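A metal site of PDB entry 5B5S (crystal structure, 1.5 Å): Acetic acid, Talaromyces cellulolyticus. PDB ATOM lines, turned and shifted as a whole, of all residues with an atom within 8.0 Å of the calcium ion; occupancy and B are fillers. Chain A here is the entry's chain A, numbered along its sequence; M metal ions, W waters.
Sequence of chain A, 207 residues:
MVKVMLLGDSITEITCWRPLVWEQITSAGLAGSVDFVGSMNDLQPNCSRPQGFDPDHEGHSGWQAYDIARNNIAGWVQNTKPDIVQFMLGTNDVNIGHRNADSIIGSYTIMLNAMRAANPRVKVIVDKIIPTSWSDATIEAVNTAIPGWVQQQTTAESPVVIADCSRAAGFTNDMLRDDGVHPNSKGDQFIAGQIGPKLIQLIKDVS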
ATOM      1  N   MET A   1     -20.756 -35.700   2.984  1.00  0.00           N
ATOM      2  CA  MET A   1     -19.851 -34.838   3.693  1.00  0.00           C
ATOM      3  C   MET A   1     -20.286 -34.709   5.152  1.00  0.00           C
ATOM      4  O   MET A   1     -21.492 -34.809   5.482  1.00  0.00           O
ATOM      5  CB  MET A   1     -19.773 -33.471   3.005  1.00  0.00           C
ATOM      6  CG  MET A   1     -19.093 -33.542   1.631  1.00  0.00           C
ATOM      7  SD  MET A   1     -18.699 -31.879   1.210  1.00  0.00           S
ATOM      8  CE  MET A   1     -20.276 -31.261   0.619  1.00  0.00           C
ATOM      9  N   LYS A   3     -21.228 -32.474   8.069  1.00  0.00           N
ATOM     10  CA  LYS A   3     -21.767 -31.139   8.253  1.00  0.00           C
ATOM     11  C   LYS A   3     -21.473 -30.562   9.600  1.00  0.00           C
ATOM     12  O   LYS A   3     -21.804 -31.136  10.673  1.00  0.00           O
ATOM     13  CB  LYS A   3     -23.283 -31.138   7.994  1.00  0.00           C
ATOM     14  CG  LYS A   3     -23.640 -31.416   6.538  1.00  0.00           C
ATOM     15  CD  LYS A   3     -25.148 -31.468   6.420  1.00  0.00           C
ATOM     16  CE  LYS A   3     -25.612 -32.781   6.996  1.00  0.00           C
ATOM     17  NZ  LYS A   3     -27.051 -32.771   7.047  1.00  0.00           N
ATOM     18  N   VAL A   4     -20.793 -29.391   9.559  1.00  0.00           N
ATOM     19  CA  VAL A   4     -20.334 -28.742  10.786  1.00  0.00           C
ATOM     20  C   VAL A   4     -20.947 -27.353  10.888  1.00  0.00           C
ATOM     21  O   VAL A   4     -20.828 -26.535   9.949  1.00  0.00           O
ATOM     22  CB  VAL A   4     -18.795 -28.575  10.711  1.00  0.00           C
ATOM     23  CG1 VAL A   4     -18.265 -27.829  11.929  1.00  0.00           C
ATOM     24  CG2 VAL A   4     -18.061 -29.893  10.609  1.00  0.00           C
ATOM     25  N   TRP A  22     -10.337 -23.817   8.803  1.00  0.00           N
ATOM     26  CA  TRP A  22     -10.540 -24.466   7.499  1.00  0.00           C
ATOM     27  C   TRP A  22      -9.151 -24.945   6.932  1.00  0.00           C
ATOM     28  O   TRP A  22      -9.062 -25.996   6.309  1.00  0.00           O
ATOM     29  CB  TRP A  22     -11.211 -23.464   6.528  1.00  0.00           C
ATOM     30  CG  TRP A  22     -11.432 -24.111   5.248  1.00  0.00           C
ATOM     31  CD1 TRP A  22     -10.668 -23.951   4.106  1.00  0.00           C
ATOM     32  CD2 TRP A  22     -12.420 -25.091   4.916  1.00  0.00           C
ATOM     33  NE1 TRP A  22     -11.137 -24.757   3.099  1.00  0.00           N
ATOM     34  CE2 TRP A  22     -12.192 -25.490   3.568  1.00  0.00           C
ATOM     35  CE3 TRP A  22     -13.450 -25.739   5.641  1.00  0.00           C
ATOM     36  CZ2 TRP A  22     -12.996 -26.479   2.903  1.00  0.00           C
ATOM     37  CZ3 TRP A  22     -14.245 -26.699   4.955  1.00  0.00           C
ATOM     38  CH2 TRP A  22     -14.026 -27.038   3.619  1.00  0.00           C
ATOM     39  N   VAL A  34     -15.861 -32.173   4.291  1.00  0.00           N
ATOM     40  CA  VAL A  34     -16.412 -31.305   5.295  1.00  0.00           C
ATOM     41  C   VAL A  34     -17.179 -30.220   4.595  1.00  0.00           C
ATOM     42  O   VAL A  34     -16.659 -29.559   3.675  1.00  0.00           O
ATOM     43  CB  VAL A  34     -15.348 -30.632   6.214  1.00  0.00           C
ATOM     44  CG1 VAL A  34     -15.951 -29.594   7.167  1.00  0.00           C
ATOM     45  CG2 VAL A  34     -14.557 -31.685   6.999  1.00  0.00           C
ATOM     46  N   ASP A  35     -18.405 -30.031   5.067  1.00  0.00           N
ATOM     47  CA  ASP A  35     -19.248 -28.895   4.635  1.00  0.00           C
ATOM     48  C   ASP A  35     -19.617 -28.063   5.895  1.00  0.00           C
ATOM     49  O   ASP A  35     -20.306 -28.541   6.797  1.00  0.00           O
ATOM     50  CB  ASP A  35     -20.565 -29.443   4.032  1.00  0.00           C
ATOM     51  CG  ASP A  35     -21.436 -28.368   3.451  1.00  0.00           C
ATOM     52  OD1 ASP A  35     -20.977 -27.216   3.220  1.00  0.00           O
ATOM     53  OD2 ASP A  35     -22.614 -28.684   3.185  1.00  0.00           O
ATOM     54  N   PHE A  36     -19.070 -26.842   5.986  1.00  0.00           N
ATOM     55  CA  PHE A  36     -19.530 -25.900   7.014  1.00  0.00           C
ATOM     56  C   PHE A  36     -20.919 -25.365   6.575  1.00  0.00           C
ATOM     57  O   PHE A  36     -21.145 -25.032   5.418  1.00  0.00           O
ATOM     58  CB  PHE A  36     -18.621 -24.686   7.128  1.00  0.00           C
ATOM     59  CG  PHE A  36     -17.269 -24.908   7.761  1.00  0.00           C
ATOM     60  CD1 PHE A  36     -16.894 -26.092   8.271  1.00  0.00           C
ATOM     61  CD2 PHE A  36     -16.364 -23.858   7.855  1.00  0.00           C
ATOM     62  CE1 PHE A  36     -15.708 -26.239   8.972  1.00  0.00           C
ATOM     63  CE2 PHE A  36     -15.143 -24.033   8.458  1.00  0.00           C
ATOM     64  CZ  PHE A  36     -14.803 -25.236   9.049  1.00  0.00           C
ATOM     65  N   VAL A  37     -21.854 -25.395   7.496  1.00  0.00           N
ATOM     66  CA  VAL A  37     -23.254 -25.045   7.267  1.00  0.00           C
ATOM     67  C   VAL A  37     -23.693 -23.938   8.281  1.00  0.00           C
ATOM     68  O   VAL A  37     -23.124 -23.779   9.383  1.00  0.00           O
ATOM     69  CB  VAL A  37     -24.186 -26.245   7.459  1.00  0.00           C
ATOM     70  CG1 VAL A  37     -23.779 -27.331   6.422  1.00  0.00           C
ATOM     71  CG2 VAL A  37     -24.268 -26.812   8.897  1.00  0.00           C
ATOM     72  N   GLY A  38     -24.710 -23.199   7.837  1.00  0.00           N
ATOM     73  CA  GLY A  38     -25.282 -22.170   8.614  1.00  0.00           C
ATOM     74  C   GLY A  38     -25.787 -21.060   7.740  1.00  0.00           C
ATOM     75  O   GLY A  38     -25.529 -21.030   6.499  1.00  0.00           O
ATOM     76  N   MET A  40     -25.401 -17.833   7.651  1.00  0.00           N
ATOM     77  CA  MET A  40     -24.564 -16.670   7.364  1.00  0.00           C
ATOM     78  C   MET A  40     -23.401 -17.046   6.483  1.00  0.00           C
ATOM     79  O   MET A  40     -22.980 -18.194   6.491  1.00  0.00           O
ATOM     80  CB  MET A  40     -24.073 -16.074   8.644  1.00  0.00           C
ATOM     81  CG  MET A  40     -25.225 -15.555   9.514  1.00  0.00           C
ATOM     82  SD  MET A  40     -25.934 -13.980   9.070  1.00  0.00           S
ATOM     83  CE  MET A  40     -24.693 -12.867   9.654  1.00  0.00           C
ATOM     84  N   ASN A  41     -22.825 -16.076   5.815  1.00  0.00           N
ATOM     85  CA  ASN A  41     -21.623 -16.385   5.096  1.00  0.00           C
ATOM     86  C   ASN A  41     -20.629 -15.245   4.942  1.00  0.00           C
ATOM     87  O   ASN A  41     -19.731 -15.313   4.115  1.00  0.00           O
ATOM     88  CB  ASN A  41     -21.950 -17.030   3.704  1.00  0.00           C
ATOM     89  CG  ASN A  41     -22.543 -16.021   2.710  1.00  0.00           C
ATOM     90  OD1 ASN A  41     -22.657 -14.857   3.003  1.00  0.00           O
ATOM     91  ND2 ASN A  41     -22.997 -16.506   1.555  1.00  0.00           N
ATOM     92  N   PHE A  53     -11.997 -21.838   0.846  1.00  0.00           N
ATOM     93  CA  PHE A  53     -12.680 -21.593   2.126  1.00  0.00           C
ATOM     94  C   PHE A  53     -14.179 -21.782   2.030  1.00  0.00           C
ATOM     95  O   PHE A  53     -14.860 -21.274   1.152  1.00  0.00           O
ATOM     96  CB  PHE A  53     -12.383 -20.177   2.601  1.00  0.00           C
ATOM     97  CG  PHE A  53     -13.014 -19.835   3.903  1.00  0.00           C
ATOM     98  CD1 PHE A  53     -12.774 -20.591   5.019  1.00  0.00           C
ATOM     99  CD2 PHE A  53     -13.820 -18.712   3.989  1.00  0.00           C
ATOM    100  CE1 PHE A  53     -13.318 -20.212   6.246  1.00  0.00           C
ATOM    101  CE2 PHE A  53     -14.346 -18.317   5.200  1.00  0.00           C
ATOM    102  CZ  PHE A  53     -14.115 -19.099   6.328  1.00  0.00           C
ATOM    103  N   ASP A  54     -14.729 -22.522   2.965  1.00  0.00           N
ATOM    104  CA  ASP A  54     -16.166 -22.653   3.080  1.00  0.00           C
ATOM    105  C   ASP A  54     -16.616 -21.526   4.070  1.00  0.00           C
ATOM    106  O   ASP A  54     -16.316 -21.601   5.247  1.00  0.00           O
ATOM    107  CB  ASP A  54     -16.534 -24.044   3.570  1.00  0.00           C
ATOM    108  CG  ASP A  54     -18.022 -24.319   3.505  1.00  0.00           C
ATOM    109  OD1 ASP A  54     -18.828 -23.340   3.633  1.00  0.00           O
ATOM    110  OD2 ASP A  54     -18.426 -25.471   3.445  1.00  0.00           O
ATOM    111  N   PRO A  55     -17.383 -20.541   3.579  1.00  0.00           N
ATOM    112  CA  PRO A  55     -17.706 -19.384   4.307  1.00  0.00           C
ATOM    113  C   PRO A  55     -18.914 -19.459   5.170  1.00  0.00           C
ATOM    114  O   PRO A  55     -19.190 -18.485   5.870  1.00  0.00           O
ATOM    115  CB  PRO A  55     -17.933 -18.340   3.191  1.00  0.00           C
ATOM    116  CG  PRO A  55     -18.598 -19.080   2.079  1.00  0.00           C
ATOM    117  CD  PRO A  55     -17.963 -20.477   2.197  1.00  0.00           C
ATOM    118  N   ASP A  56     -19.646 -20.574   5.150  1.00  0.00           N
ATOM    119  CA  ASP A  56     -20.909 -20.648   5.930  1.00  0.00           C
ATOM    120  C   ASP A  56     -20.643 -20.811   7.429  1.00  0.00           C
ATOM    121  O   ASP A  56     -19.757 -21.507   7.852  1.00  0.00           O
ATOM    122  CB  ASP A  56     -21.726 -21.779   5.416  1.00  0.00           C
ATOM    123  CG  ASP A  56     -22.040 -21.630   3.958  1.00  0.00           C
ATOM    124  OD1 ASP A  56     -22.491 -20.534   3.547  1.00  0.00           O
ATOM    125  OD2 ASP A  56     -21.875 -22.631   3.253  1.00  0.00           O
ATOM    126  N   HIS A  57     -21.449 -20.115   8.199  1.00  0.00           N
ATOM    127  CA  HIS A  57     -21.416 -20.051   9.622  1.00  0.00           C
ATOM    128  C   HIS A  57     -22.774 -19.646  10.213  1.00  0.00           C
ATOM    129  O   HIS A  57     -23.708 -19.188   9.489  1.00  0.00           O
ATOM    130  CB  HIS A  57     -20.271 -19.145  10.111  1.00  0.00           C
ATOM    131  CG  HIS A  57     -20.472 -17.711   9.836  1.00  0.00           C
ATOM    132  ND1 HIS A  57     -21.101 -16.857  10.711  1.00  0.00           N
ATOM    133  CD2 HIS A  57     -20.036 -16.951   8.828  1.00  0.00           C
ATOM    134  CE1 HIS A  57     -21.105 -15.645  10.214  1.00  0.00           C
ATOM    135  NE2 HIS A  57     -20.504 -15.676   9.052  1.00  0.00           N
HETATM  136 CA    CA M   1     -20.827 -24.814   3.185  1.00  0.00          CA
HETATM  137  O   HOH W   1     -20.236 -24.597   0.790  1.00  0.00           O
HETATM  138  O   HOH W   2     -23.173 -25.233   2.797  1.00  0.00           O
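The backbone NH of Val 4 lies within hydrogen-bond range of the backbone carbonyl oxygen of Asp 35.
The calcium ion is bound by O of Phe 36 (2.3 Å), OD1 of Asp 35 (2.4 Å), water W2 (2.4 Å), OD2 of Asp 56 (2.4 Å), water W1 (2.5 Å), OD2 of Asp 54 (2.5 Å) and OD1 of Asp 54 (2.5 Å).
The nearest printed residue that does not touch the calcium ion is Val 37 (4.5 Å).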
